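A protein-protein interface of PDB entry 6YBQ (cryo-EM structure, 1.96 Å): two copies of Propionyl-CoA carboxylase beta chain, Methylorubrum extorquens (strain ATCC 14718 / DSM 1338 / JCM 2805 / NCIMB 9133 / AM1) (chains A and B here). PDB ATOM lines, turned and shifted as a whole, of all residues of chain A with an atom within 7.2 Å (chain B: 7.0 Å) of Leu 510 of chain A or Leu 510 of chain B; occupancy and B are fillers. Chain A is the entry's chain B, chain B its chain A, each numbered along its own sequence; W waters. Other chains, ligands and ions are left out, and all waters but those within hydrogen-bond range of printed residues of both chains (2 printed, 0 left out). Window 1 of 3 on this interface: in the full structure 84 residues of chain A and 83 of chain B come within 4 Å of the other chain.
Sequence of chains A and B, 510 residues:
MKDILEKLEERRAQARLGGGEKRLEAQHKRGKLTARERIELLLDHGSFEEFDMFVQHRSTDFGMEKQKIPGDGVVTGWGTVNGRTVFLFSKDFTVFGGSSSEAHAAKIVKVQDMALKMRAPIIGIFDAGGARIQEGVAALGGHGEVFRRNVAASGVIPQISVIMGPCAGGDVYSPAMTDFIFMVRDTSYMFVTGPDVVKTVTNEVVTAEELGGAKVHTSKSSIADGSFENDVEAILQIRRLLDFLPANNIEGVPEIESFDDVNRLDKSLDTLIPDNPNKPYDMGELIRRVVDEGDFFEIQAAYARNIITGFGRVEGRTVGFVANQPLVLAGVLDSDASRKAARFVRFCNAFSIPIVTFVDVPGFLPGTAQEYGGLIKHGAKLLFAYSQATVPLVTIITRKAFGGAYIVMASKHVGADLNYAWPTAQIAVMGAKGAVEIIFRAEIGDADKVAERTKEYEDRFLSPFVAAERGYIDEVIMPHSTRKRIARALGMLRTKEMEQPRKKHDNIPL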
ATOM      1  N   SER A 222     -14.857  -9.188  -1.515  1.00  0.00           N
ATOM      2  CA  SER A 222     -13.494  -8.697  -1.265  1.00  0.00           C
ATOM      3  C   SER A 222     -12.987  -8.948   0.153  1.00  0.00           C
ATOM      4  O   SER A 222     -11.887  -8.487   0.484  1.00  0.00           O
ATOM      5  CB  SER A 222     -13.364  -7.194  -1.524  1.00  0.00           C
ATOM      6  OG  SER A 222     -13.801  -6.470  -0.396  1.00  0.00           O
ATOM      7  N   SER A 338      -7.733  -3.229  -8.611  1.00  0.00           N
ATOM      8  CA  SER A 338      -6.967  -2.119  -8.050  1.00  0.00           C
ATOM      9  C   SER A 338      -6.899  -2.222  -6.533  1.00  0.00           C
ATOM     10  O   SER A 338      -5.826  -2.104  -5.936  1.00  0.00           O
ATOM     11  CB  SER A 338      -7.584  -0.781  -8.475  1.00  0.00           C
ATOM     12  OG  SER A 338      -7.741  -0.698  -9.877  1.00  0.00           O
ATOM     13  N   ARG A 339      -8.042  -2.469  -5.893  1.00  0.00           N
ATOM     14  CA  ARG A 339      -8.073  -2.578  -4.439  1.00  0.00           C
ATOM     15  C   ARG A 339      -7.267  -3.788  -3.961  1.00  0.00           C
ATOM     16  O   ARG A 339      -6.461  -3.684  -3.016  1.00  0.00           O
ATOM     17  CB  ARG A 339      -9.530  -2.651  -3.972  1.00  0.00           C
ATOM     18  CG  ARG A 339     -10.336  -1.389  -4.258  1.00  0.00           C
ATOM     19  CD  ARG A 339     -11.810  -1.591  -3.979  1.00  0.00           C
ATOM     20  NE  ARG A 339     -12.023  -2.114  -2.636  1.00  0.00           N
ATOM     21  CZ  ARG A 339     -12.970  -2.983  -2.304  1.00  0.00           C
ATOM     22  NH1 ARG A 339     -13.829  -3.432  -3.206  1.00  0.00           N
ATOM     23  NH2 ARG A 339     -13.061  -3.396  -1.050  1.00  0.00           N
ATOM     24  N   LYS A 340      -7.476  -4.946  -4.607  1.00  0.00           N
ATOM     25  CA  LYS A 340      -6.733  -6.163  -4.278  1.00  0.00           C
ATOM     26  C   LYS A 340      -5.230  -5.914  -4.284  1.00  0.00           C
ATOM     27  O   LYS A 340      -4.522  -6.285  -3.341  1.00  0.00           O
ATOM     28  CB  LYS A 340      -7.096  -7.288  -5.261  1.00  0.00           C
ATOM     29  CG  LYS A 340      -6.238  -8.558  -5.170  1.00  0.00           C
ATOM     30  CD  LYS A 340      -6.762  -9.670  -6.088  1.00  0.00           C
ATOM     31  CE  LYS A 340      -5.812 -10.844  -6.234  1.00  0.00           C
ATOM     32  NZ  LYS A 340      -6.314 -11.843  -7.214  1.00  0.00           N
ATOM     33  N   ALA A 341      -4.724  -5.295  -5.351  1.00  0.00           N
ATOM     34  CA  ALA A 341      -3.285  -5.082  -5.474  1.00  0.00           C
ATOM     35  C   ALA A 341      -2.785  -4.006  -4.513  1.00  0.00           C
ATOM     36  O   ALA A 341      -1.662  -4.098  -3.999  1.00  0.00           O
ATOM     37  CB  ALA A 341      -2.936  -4.721  -6.915  1.00  0.00           C
ATOM     38  N   ALA A 342      -3.597  -2.975  -4.265  1.00  0.00           N
ATOM     39  CA  ALA A 342      -3.173  -1.880  -3.399  1.00  0.00           C
ATOM     40  C   ALA A 342      -2.941  -2.356  -1.967  1.00  0.00           C
ATOM     41  O   ALA A 342      -1.930  -2.005  -1.345  1.00  0.00           O
ATOM     42  CB  ALA A 342      -4.202  -0.752  -3.437  1.00  0.00           C
ATOM     43  N   ARG A 343      -3.877  -3.136  -1.414  1.00  0.00           N
ATOM     44  CA  ARG A 343      -3.696  -3.587  -0.029  1.00  0.00           C
ATOM     45  C   ARG A 343      -2.419  -4.411   0.107  1.00  0.00           C
ATOM     46  O   ARG A 343      -1.668  -4.260   1.079  1.00  0.00           O
ATOM     47  CB  ARG A 343      -4.910  -4.384   0.458  1.00  0.00           C
ATOM     48  CG  ARG A 343      -4.910  -4.726   1.972  1.00  0.00           C
ATOM     49  CD  ARG A 343      -5.841  -3.818   2.759  1.00  0.00           C
ATOM     50  NE  ARG A 343      -5.628  -3.842   4.209  1.00  0.00           N
ATOM     51  CZ  ARG A 343      -6.166  -4.721   5.047  1.00  0.00           C
ATOM     52  NH1 ARG A 343      -6.961  -5.682   4.606  1.00  0.00           N
ATOM     53  NH2 ARG A 343      -5.908  -4.639   6.344  1.00  0.00           N
ATOM     54  N   PHE A 344      -2.144  -5.259  -0.884  1.00  0.00           N
ATOM     55  CA  PHE A 344      -0.939  -6.082  -0.884  1.00  0.00           C
ATOM     56  C   PHE A 344       0.325  -5.228  -0.939  1.00  0.00           C
ATOM     57  O   PHE A 344       1.292  -5.479  -0.206  1.00  0.00           O
ATOM     58  CB  PHE A 344      -1.003  -7.055  -2.064  1.00  0.00           C
ATOM     59  CG  PHE A 344       0.060  -8.106  -2.048  1.00  0.00           C
ATOM     60  CD1 PHE A 344      -0.044  -9.204  -1.216  1.00  0.00           C
ATOM     61  CD2 PHE A 344       1.160  -8.004  -2.874  1.00  0.00           C
ATOM     62  CE1 PHE A 344       0.933 -10.167  -1.208  1.00  0.00           C
ATOM     63  CE2 PHE A 344       2.133  -8.963  -2.864  1.00  0.00           C
ATOM     64  CZ  PHE A 344       2.019 -10.044  -2.031  1.00  0.00           C
ATOM     65  N   ARG A 346       0.665  -2.190   0.060  1.00  0.00           N
ATOM     66  CA  ARG A 346       0.791  -1.490   1.337  1.00  0.00           C
ATOM     67  C   ARG A 346       1.349  -2.416   2.417  1.00  0.00           C
ATOM     68  O   ARG A 346       2.251  -2.030   3.173  1.00  0.00           O
ATOM     69  CB  ARG A 346      -0.562  -0.912   1.758  1.00  0.00           C
ATOM     70  CG  ARG A 346      -1.072   0.253   0.897  1.00  0.00           C
ATOM     71  CD  ARG A 346      -0.818   1.604   1.518  1.00  0.00           C
ATOM     72  NE  ARG A 346      -1.644   1.838   2.700  1.00  0.00           N
ATOM     73  CZ  ARG A 346      -1.683   2.981   3.370  1.00  0.00           C
ATOM     74  NH1 ARG A 346      -0.957   4.014   2.977  1.00  0.00           N
ATOM     75  NH2 ARG A 346      -2.461   3.093   4.434  1.00  0.00           N
ATOM     76  N   GLY A 374     -17.102   4.221  -8.961  1.00  0.00           N
ATOM     77  CA  GLY A 374     -16.014   4.994  -8.412  1.00  0.00           C
ATOM     78  C   GLY A 374     -14.627   4.644  -8.903  1.00  0.00           C
ATOM     79  O   GLY A 374     -13.669   4.790  -8.138  1.00  0.00           O
ATOM     80  N   LYS A 377     -11.370   6.773  -8.109  1.00  0.00           N
ATOM     81  CA  LYS A 377     -10.660   6.728  -6.831  1.00  0.00           C
ATOM     82  C   LYS A 377     -10.079   5.343  -6.527  1.00  0.00           C
ATOM     83  O   LYS A 377      -8.934   5.230  -6.050  1.00  0.00           O
ATOM     84  CB  LYS A 377     -11.599   7.193  -5.708  1.00  0.00           C
ATOM     85  CG  LYS A 377     -11.616   8.716  -5.532  1.00  0.00           C
ATOM     86  CD  LYS A 377     -12.332   9.162  -4.272  1.00  0.00           C
ATOM     87  CE  LYS A 377     -12.607  10.657  -4.283  1.00  0.00           C
ATOM     88  NZ  LYS A 377     -13.489  11.068  -3.164  1.00  0.00           N
ATOM     89  N   HIS A 378     -10.846   4.284  -6.799  1.00  0.00           N
ATOM     90  CA  HIS A 378     -10.323   2.931  -6.648  1.00  0.00           C
ATOM     91  C   HIS A 378      -9.056   2.740  -7.473  1.00  0.00           C
ATOM     92  O   HIS A 378      -8.080   2.153  -6.998  1.00  0.00           O
ATOM     93  CB  HIS A 378     -11.392   1.911  -7.043  1.00  0.00           C
ATOM     94  CG  HIS A 378     -12.643   1.998  -6.229  1.00  0.00           C
ATOM     95  ND1 HIS A 378     -12.633   2.176  -4.864  1.00  0.00           N
ATOM     96  CD2 HIS A 378     -13.946   1.933  -6.588  1.00  0.00           C
ATOM     97  CE1 HIS A 378     -13.873   2.217  -4.416  1.00  0.00           C
ATOM     98  NE2 HIS A 378     -14.690   2.071  -5.442  1.00  0.00           N
ATOM     99  N   LYS A 381      -5.988   4.354  -5.837  1.00  0.00           N
ATOM    100  CA  LYS A 381      -5.411   3.693  -4.663  1.00  0.00           C
ATOM    101  C   LYS A 381      -4.112   2.956  -5.002  1.00  0.00           C
ATOM    102  O   LYS A 381      -3.139   3.025  -4.244  1.00  0.00           O
ATOM    103  CB  LYS A 381      -6.424   2.734  -4.045  1.00  0.00           C
ATOM    104  CG  LYS A 381      -7.693   3.407  -3.543  1.00  0.00           C
ATOM    105  CD  LYS A 381      -8.757   2.408  -3.168  1.00  0.00           C
ATOM    106  CE  LYS A 381      -9.977   3.089  -2.577  1.00  0.00           C
ATOM    107  NZ  LYS A 381     -10.946   2.109  -2.041  1.00  0.00           N
ATOM    108  N   LEU A 382      -4.074   2.245  -6.134  1.00  0.00           N
ATOM    109  CA  LEU A 382      -2.868   1.506  -6.522  1.00  0.00           C
ATOM    110  C   LEU A 382      -1.718   2.446  -6.876  1.00  0.00           C
ATOM    111  O   LEU A 382      -0.563   2.205  -6.494  1.00  0.00           O
ATOM    112  CB  LEU A 382      -3.176   0.570  -7.698  1.00  0.00           C
ATOM    113  CG  LEU A 382      -2.099  -0.426  -8.141  1.00  0.00           C
ATOM    114  CD1 LEU A 382      -1.565  -1.231  -6.970  1.00  0.00           C
ATOM    115  CD2 LEU A 382      -2.625  -1.346  -9.240  1.00  0.00           C
ATOM    116  N   ALA A 385      -0.354   3.683  -3.654  1.00  0.00           N
ATOM    117  CA  ALA A 385       0.417   2.666  -2.942  1.00  0.00           C
ATOM    118  C   ALA A 385       1.816   2.520  -3.527  1.00  0.00           C
ATOM    119  O   ALA A 385       2.806   2.477  -2.790  1.00  0.00           O
ATOM    120  CB  ALA A 385      -0.315   1.324  -2.968  1.00  0.00           C
ATOM    121  N   ASN A 507      -3.376  10.889   3.349  1.00  0.00           N
ATOM    122  CA  ASN A 507      -4.822  10.968   3.160  1.00  0.00           C
ATOM    123  C   ASN A 507      -5.236  10.173   1.926  1.00  0.00           C
ATOM    124  O   ASN A 507      -5.982  10.667   1.076  1.00  0.00           O
ATOM    125  CB  ASN A 507      -5.289  12.419   3.045  1.00  0.00           C
ATOM    126  CG  ASN A 507      -6.801  12.543   3.083  1.00  0.00           C
ATOM    127  OD1 ASN A 507      -7.497  11.660   3.581  1.00  0.00           O
ATOM    128  ND2 ASN A 507      -7.314  13.639   2.553  1.00  0.00           N
ATOM    129  N   ILE A 508      -4.728   8.950   1.813  1.00  0.00           N
ATOM    130  CA  ILE A 508      -5.046   8.049   0.708  1.00  0.00           C
ATOM    131  C   ILE A 508      -6.563   7.974   0.572  1.00  0.00           C
ATOM    132  O   ILE A 508      -7.264   7.912   1.591  1.00  0.00           O
ATOM    133  CB  ILE A 508      -4.431   6.656   0.932  1.00  0.00           C
ATOM    134  CG1 ILE A 508      -4.525   5.809  -0.342  1.00  0.00           C
ATOM    135  CG2 ILE A 508      -5.086   5.962   2.116  1.00  0.00           C
ATOM    136  CD1 ILE A 508      -3.898   4.438  -0.236  1.00  0.00           C
ATOM    137  N   PRO A 509      -7.118   7.985  -0.638  1.00  0.00           N
ATOM    138  CA  PRO A 509      -8.576   7.911  -0.768  1.00  0.00           C
ATOM    139  C   PRO A 509      -9.118   6.572  -0.297  1.00  0.00           C
ATOM    140  O   PRO A 509      -8.430   5.550  -0.322  1.00  0.00           O
ATOM    141  CB  PRO A 509      -8.817   8.119  -2.267  1.00  0.00           C
ATOM    142  CG  PRO A 509      -7.533   7.854  -2.918  1.00  0.00           C
ATOM    143  CD  PRO A 509      -6.462   8.170  -1.944  1.00  0.00           C
ATOM    144  N   LEU A 510     -10.372   6.593   0.143  1.00  0.00           N
ATOM    145  CA  LEU A 510     -11.022   5.405   0.689  1.00  0.00           C
ATOM    146  C   LEU A 510     -12.270   5.027  -0.106  1.00  0.00           C
ATOM    147  O   LEU A 510     -12.568   5.615  -1.144  1.00  0.00           O
ATOM    148  CB  LEU A 510     -11.393   5.628   2.156  1.00  0.00           C
ATOM    149  CG  LEU A 510     -10.243   5.955   3.104  1.00  0.00           C
ATOM    150  CD1 LEU A 510     -10.759   6.156   4.514  1.00  0.00           C
ATOM    151  CD2 LEU A 510      -9.211   4.851   3.060  1.00  0.00           C
ATOM    152  OXT LEU A 510     -13.010   4.118   0.269  1.00  0.00           O
ATOM    153  N   SER B 222     -19.382   8.964  -5.394  1.00  0.00           N
ATOM    154  CA  SER B 222     -18.552   9.323  -4.236  1.00  0.00           C
ATOM    155  C   SER B 222     -17.332  10.169  -4.586  1.00  0.00           C
ATOM    156  O   SER B 222     -16.495  10.410  -3.709  1.00  0.00           O
ATOM    157  CB  SER B 222     -18.068   8.077  -3.486  1.00  0.00           C
ATOM    158  OG  SER B 222     -17.158   7.323  -4.263  1.00  0.00           O
ATOM    159  N   SER B 338     -20.172   5.342   5.789  1.00  0.00           N
ATOM    160  CA  SER B 338     -18.936   5.010   6.486  1.00  0.00           C
ATOM    161  C   SER B 338     -17.725   5.577   5.754  1.00  0.00           C
ATOM    162  O   SER B 338     -16.856   6.202   6.369  1.00  0.00           O
ATOM    163  CB  SER B 338     -18.821   3.497   6.657  1.00  0.00           C
ATOM    164  OG  SER B 338     -19.810   3.019   7.547  1.00  0.00           O
ATOM    165  N   ARG B 339     -17.655   5.377   4.436  1.00  0.00           N
ATOM    166  CA  ARG B 339     -16.535   5.925   3.669  1.00  0.00           C
ATOM    167  C   ARG B 339     -16.515   7.454   3.745  1.00  0.00           C
ATOM    168  O   ARG B 339     -15.462   8.074   3.991  1.00  0.00           O
ATOM    169  CB  ARG B 339     -16.620   5.428   2.221  1.00  0.00           C
ATOM    170  CG  ARG B 339     -16.250   3.951   2.053  1.00  0.00           C
ATOM    171  CD  ARG B 339     -16.357   3.449   0.618  1.00  0.00           C
ATOM    172  NE  ARG B 339     -15.772   4.384  -0.334  1.00  0.00           N
ATOM    173  CZ  ARG B 339     -16.204   4.567  -1.577  1.00  0.00           C
ATOM    174  NH1 ARG B 339     -17.234   3.879  -2.048  1.00  0.00           N
ATOM    175  NH2 ARG B 339     -15.596   5.446  -2.355  1.00  0.00           N
ATOM    176  N   LYS B 340     -17.687   8.075   3.554  1.00  0.00           N
ATOM    177  CA  LYS B 340     -17.809   9.530   3.631  1.00  0.00           C
ATOM    178  C   LYS B 340     -17.237  10.062   4.938  1.00  0.00           C
ATOM    179  O   LYS B 340     -16.462  11.022   4.945  1.00  0.00           O
ATOM    180  CB  LYS B 340     -19.284   9.942   3.467  1.00  0.00           C
ATOM    181  CG  LYS B 340     -19.607  11.409   3.759  1.00  0.00           C
ATOM    182  CD  LYS B 340     -21.042  11.789   3.356  1.00  0.00           C
ATOM    183  CE  LYS B 340     -21.434  13.202   3.779  1.00  0.00           C
ATOM    184  NZ  LYS B 340     -22.867  13.492   3.510  1.00  0.00           N
ATOM    185  N   ALA B 341     -17.604   9.439   6.059  1.00  0.00           N
ATOM    186  CA  ALA B 341     -17.157   9.929   7.361  1.00  0.00           C
ATOM    187  C   ALA B 341     -15.680   9.619   7.603  1.00  0.00           C
ATOM    188  O   ALA B 341     -14.957  10.431   8.197  1.00  0.00           O
ATOM    189  CB  ALA B 341     -18.030   9.333   8.465  1.00  0.00           C
ATOM    190  N   ALA B 342     -15.215   8.452   7.153  1.00  0.00           N
ATOM    191  CA  ALA B 342     -13.846   8.027   7.435  1.00  0.00           C
ATOM    192  C   ALA B 342     -12.829   8.967   6.794  1.00  0.00           C
ATOM    193  O   ALA B 342     -11.848   9.369   7.437  1.00  0.00           O
ATOM    194  CB  ALA B 342     -13.632   6.588   6.960  1.00  0.00           C
ATOM    195  N   ARG B 343     -13.046   9.342   5.529  1.00  0.00           N
ATOM    196  CA  ARG B 343     -12.064  10.228   4.892  1.00  0.00           C
ATOM    197  C   ARG B 343     -12.037  11.612   5.549  1.00  0.00           C
ATOM    198  O   ARG B 343     -10.964  12.208   5.716  1.00  0.00           O
ATOM    199  CB  ARG B 343     -12.315  10.355   3.389  1.00  0.00           C
ATOM    200  CG  ARG B 343     -11.164  11.064   2.651  1.00  0.00           C
ATOM    201  CD  ARG B 343     -10.763  10.371   1.369  1.00  0.00           C
ATOM    202  NE  ARG B 343      -9.464  10.823   0.868  1.00  0.00           N
ATOM    203  CZ  ARG B 343      -9.289  11.657  -0.150  1.00  0.00           C
ATOM    204  NH1 ARG B 343     -10.324  12.169  -0.794  1.00  0.00           N
ATOM    205  NH2 ARG B 343      -8.064  11.987  -0.523  1.00  0.00           N
ATOM    206  N   PHE B 344     -13.204  12.140   5.927  1.00  0.00           N
ATOM    207  CA  PHE B 344     -13.266  13.432   6.607  1.00  0.00           C
ATOM    208  C   PHE B 344     -12.529  13.396   7.943  1.00  0.00           C
ATOM    209  O   PHE B 344     -11.779  14.326   8.275  1.00  0.00           O
ATOM    210  CB  PHE B 344     -14.729  13.843   6.799  1.00  0.00           C
ATOM    211  CG  PHE B 344     -14.914  15.215   7.384  1.00  0.00           C
ATOM    212  CD1 PHE B 344     -14.816  16.342   6.591  1.00  0.00           C
ATOM    213  CD2 PHE B 344     -15.206  15.378   8.723  1.00  0.00           C
ATOM    214  CE1 PHE B 344     -14.992  17.597   7.132  1.00  0.00           C
ATOM    215  CE2 PHE B 344     -15.383  16.632   9.257  1.00  0.00           C
ATOM    216  CZ  PHE B 344     -15.276  17.738   8.460  1.00  0.00           C
ATOM    217  N   ARG B 346     -10.089  11.394   8.769  1.00  0.00           N
ATOM    218  CA  ARG B 346      -8.661  11.302   8.482  1.00  0.00           C
ATOM    219  C   ARG B 346      -8.084  12.671   8.130  1.00  0.00           C
ATOM    220  O   ARG B 346      -7.007  13.041   8.614  1.00  0.00           O
ATOM    221  CB  ARG B 346      -8.419  10.292   7.360  1.00  0.00           C
ATOM    222  CG  ARG B 346      -8.729   8.838   7.735  1.00  0.00           C
ATOM    223  CD  ARG B 346      -7.501   8.064   8.131  1.00  0.00           C
ATOM    224  NE  ARG B 346      -6.617   7.838   6.993  1.00  0.00           N
ATOM    225  CZ  ARG B 346      -5.542   7.061   7.020  1.00  0.00           C
ATOM    226  NH1 ARG B 346      -5.208   6.414   8.122  1.00  0.00           N
ATOM    227  NH2 ARG B 346      -4.802   6.928   5.935  1.00  0.00           N
ATOM    228  N   LYS B 377     -15.705  -4.412   5.769  1.00  0.00           N
ATOM    229  CA  LYS B 377     -14.514  -3.568   5.656  1.00  0.00           C
ATOM    230  C   LYS B 377     -14.873  -2.079   5.606  1.00  0.00           C
ATOM    231  O   LYS B 377     -14.208  -1.245   6.247  1.00  0.00           O
ATOM    232  CB  LYS B 377     -13.711  -3.978   4.415  1.00  0.00           C
ATOM    233  CG  LYS B 377     -12.746  -5.156   4.629  1.00  0.00           C
ATOM    234  CD  LYS B 377     -11.801  -5.369   3.436  1.00  0.00           C
ATOM    235  CE  LYS B 377     -11.076  -6.707   3.523  1.00  0.00           C
ATOM    236  NZ  LYS B 377     -10.379  -7.107   2.267  1.00  0.00           N
ATOM    237  N   HIS B 378     -15.912  -1.721   4.847  1.00  0.00           N
ATOM    238  CA  HIS B 378     -16.288  -0.314   4.722  1.00  0.00           C
ATOM    239  C   HIS B 378     -16.652   0.279   6.077  1.00  0.00           C
ATOM    240  O   HIS B 378     -16.229   1.389   6.413  1.00  0.00           O
ATOM    241  CB  HIS B 378     -17.448  -0.159   3.735  1.00  0.00           C
ATOM    242  CG  HIS B 378     -17.106  -0.548   2.331  1.00  0.00           C
ATOM    243  ND1 HIS B 378     -16.000  -0.058   1.673  1.00  0.00           N
ATOM    244  CD2 HIS B 378     -17.725  -1.376   1.458  1.00  0.00           C
ATOM    245  CE1 HIS B 378     -15.950  -0.570   0.457  1.00  0.00           C
ATOM    246  NE2 HIS B 378     -16.987  -1.372   0.301  1.00  0.00           N
ATOM    247  N   LYS B 381     -13.678   0.984   8.252  1.00  0.00           N
ATOM    248  CA  LYS B 381     -12.869   2.164   7.922  1.00  0.00           C
ATOM    249  C   LYS B 381     -13.097   3.315   8.913  1.00  0.00           C
ATOM    250  O   LYS B 381     -12.141   3.970   9.348  1.00  0.00           O
ATOM    251  CB  LYS B 381     -13.147   2.619   6.484  1.00  0.00           C
ATOM    252  CG  LYS B 381     -12.678   1.621   5.427  1.00  0.00           C
ATOM    253  CD  LYS B 381     -12.921   2.091   4.005  1.00  0.00           C
ATOM    254  CE  LYS B 381     -12.637   0.991   2.994  1.00  0.00           C
ATOM    255  NZ  LYS B 381     -13.019   1.396   1.621  1.00  0.00           N
ATOM    256  N   LEU B 382     -14.354   3.575   9.287  1.00  0.00           N
ATOM    257  CA  LEU B 382     -14.651   4.636  10.248  1.00  0.00           C
ATOM    258  C   LEU B 382     -14.140   4.293  11.646  1.00  0.00           C
ATOM    259  O   LEU B 382     -13.574   5.153  12.338  1.00  0.00           O
ATOM    260  CB  LEU B 382     -16.157   4.900  10.278  1.00  0.00           C
ATOM    261  CG  LEU B 382     -16.681   6.119  11.040  1.00  0.00           C
ATOM    262  CD1 LEU B 382     -15.987   7.409  10.634  1.00  0.00           C
ATOM    263  CD2 LEU B 382     -18.186   6.238  10.851  1.00  0.00           C
ATOM    264  N   ALA B 385     -10.495   5.129  11.507  1.00  0.00           N
ATOM    265  CA  ALA B 385     -10.179   6.552  11.508  1.00  0.00           C
ATOM    266  C   ALA B 385     -10.336   7.148  12.899  1.00  0.00           C
ATOM    267  O   ALA B 385      -9.493   7.934  13.341  1.00  0.00           O
ATOM    268  CB  ALA B 385     -11.060   7.290  10.503  1.00  0.00           C
ATOM    269  N   ASN B 507      -2.023  -0.044   7.942  1.00  0.00           N
ATOM    270  CA  ASN B 507      -2.600  -0.879   6.893  1.00  0.00           C
ATOM    271  C   ASN B 507      -4.125  -0.839   6.912  1.00  0.00           C
ATOM    272  O   ASN B 507      -4.776  -1.885   6.879  1.00  0.00           O
ATOM    273  CB  ASN B 507      -2.135  -2.330   7.005  1.00  0.00           C
ATOM    274  CG  ASN B 507      -2.415  -3.119   5.742  1.00  0.00           C
ATOM    275  OD1 ASN B 507      -2.472  -2.561   4.650  1.00  0.00           O
ATOM    276  ND2 ASN B 507      -2.612  -4.414   5.886  1.00  0.00           N
ATOM    277  N   ILE B 508      -4.700   0.356   6.991  1.00  0.00           N
ATOM    278  CA  ILE B 508      -6.149   0.550   6.939  1.00  0.00           C
ATOM    279  C   ILE B 508      -6.741  -0.257   5.786  1.00  0.00           C
ATOM    280  O   ILE B 508      -6.153  -0.286   4.697  1.00  0.00           O
ATOM    281  CB  ILE B 508      -6.493   2.045   6.807  1.00  0.00           C
ATOM    282  CG1 ILE B 508      -7.984   2.290   7.080  1.00  0.00           C
ATOM    283  CG2 ILE B 508      -6.048   2.584   5.449  1.00  0.00           C
ATOM    284  CD1 ILE B 508      -8.334   3.728   7.400  1.00  0.00           C
ATOM    285  N   PRO B 509      -7.876  -0.935   5.971  1.00  0.00           N
ATOM    286  CA  PRO B 509      -8.510  -1.616   4.836  1.00  0.00           C
ATOM    287  C   PRO B 509      -8.962  -0.624   3.777  1.00  0.00           C
ATOM    288  O   PRO B 509      -9.307   0.520   4.075  1.00  0.00           O
ATOM    289  CB  PRO B 509      -9.704  -2.343   5.465  1.00  0.00           C
ATOM    290  CG  PRO B 509      -9.863  -1.799   6.804  1.00  0.00           C
ATOM    291  CD  PRO B 509      -8.584  -1.196   7.236  1.00  0.00           C
ATOM    292  N   LEU B 510      -8.966  -1.077   2.530  1.00  0.00           N
ATOM    293  CA  LEU B 510      -9.351  -0.224   1.413  1.00  0.00           C
ATOM    294  C   LEU B 510     -10.538  -0.808   0.649  1.00  0.00           C
ATOM    295  O   LEU B 510     -10.804  -2.007   0.708  1.00  0.00           O
ATOM    296  CB  LEU B 510      -8.168  -0.021   0.466  1.00  0.00           C
ATOM    297  CG  LEU B 510      -6.883   0.484   1.116  1.00  0.00           C
ATOM    298  CD1 LEU B 510      -5.724   0.470   0.134  1.00  0.00           C
ATOM    299  CD2 LEU B 510      -7.088   1.863   1.698  1.00  0.00           C
ATOM    300  OXT LEU B 510     -11.256  -0.095  -0.051  1.00  0.00           O
HETATM  301  O   HOH W   1      -3.372  -0.153   3.674  1.00  0.00           O
HETATM  302  O   HOH W   2      -7.426   9.121   4.095  1.00  0.00           O
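Of the 19 printed residues of chain A, 10 touch a printed residue of chain B.
Among the printed residues, 18 pairs touch across the chains.
Among the printed residues, no Asp or Glu carboxylate lies within 4 Å of a Lys or Arg side-chain nitrogen of the other chain.
O of Asn 507 of chain B sits at hydrogen-bond distance from NH2 of Arg 343 of chain A (3.0 Å).
The guanidinium group (NE) of Arg 339 of chain B lies within salt-bridge range of the chain-end carboxylate (OXT) of Leu 510 of chain A, 2.8 Å away.
NH2 of Arg 339 of chain A is in salt-bridge range of O of Leu 510 of chain B (3.2 Å).
OXT of Leu 510 of chain A is in salt-bridge range of NZ of Lys 381 of chain B (3.0 Å).
O of Ser 222 of chain B lies within hydrogen-bond range of NZ of Lys 377 of chain A, 3.1 Å away.
The chain-end carboxylate (OXT) of Leu 510 of chain B lies within salt-bridge range of the side-chain amino group (NZ) of Lys 381 of chain A, 3.0 Å away.
The guanidinium group of Arg 343 of chain B is in hydrogen-bond range of the backbone carbonyl oxygen of Asn 507 of chain A (2.9 Å).
NZ of Lys 377 of chain B sits at hydrogen-bond distance from O of Ser 222 of chain A, at 2.7 Å.
Arg 343 of chain A touches Asn 507 of chain B, and with the chains exchanged Asn 507 of chain A touches Arg 343 of chain B.
Positions printed for both chains: 222, 338, 339, 340, 341, 342, 343, 344, 346, 377, 378, 381, 382, 385, 507, 508, 509 and 510.
Printed residues of chain B within 4 Å of Leu 510 of chain A: Arg 339 (2.8 Å), Ala 342 (3.8 Å), Arg 343 (3.99 Å), Lys 381 (3.0 Å) and Leu 510 (3.9 Å).
Leu 510 of chain B touches just these residues of chain A: Arg 339 (3.2 Å), Lys 381 (3.0 Å) and Leu 510 (3.9 Å).
Ala 385 of chain B touches none of the printed residues of chain A.
The nearest printed residue of chain A that does not touch Arg 343 of chain B is Lys 377 of chain A (4.1 Å).
Asn 507 of chain B touches Arg 346 of chain A.
Ile 508 of chain A touches Arg 343 of chain B.
Pro 509 of chain A touches Arg 343 of chain B (CA to NE, 3.5 Å).
CD of Arg 343 of chain B touches N of Leu 510 of chain A (3.99 Å).
The chain-end carboxylate (OXT) of Leu 510 of chain A lies within salt-bridge range of the side-chain amino group (NZ) of Lys 381 of chain A (3.7 Å).
Water W1 lies within hydrogen-bond range of the side-chain amide oxygen of Asn 507 of chain B (2.7 Å), the guanidinium group of Arg 346 of chain A (2.8 Å) and the backbone carbonyl oxygen of Ile 508 of chain B (3.0 Å).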
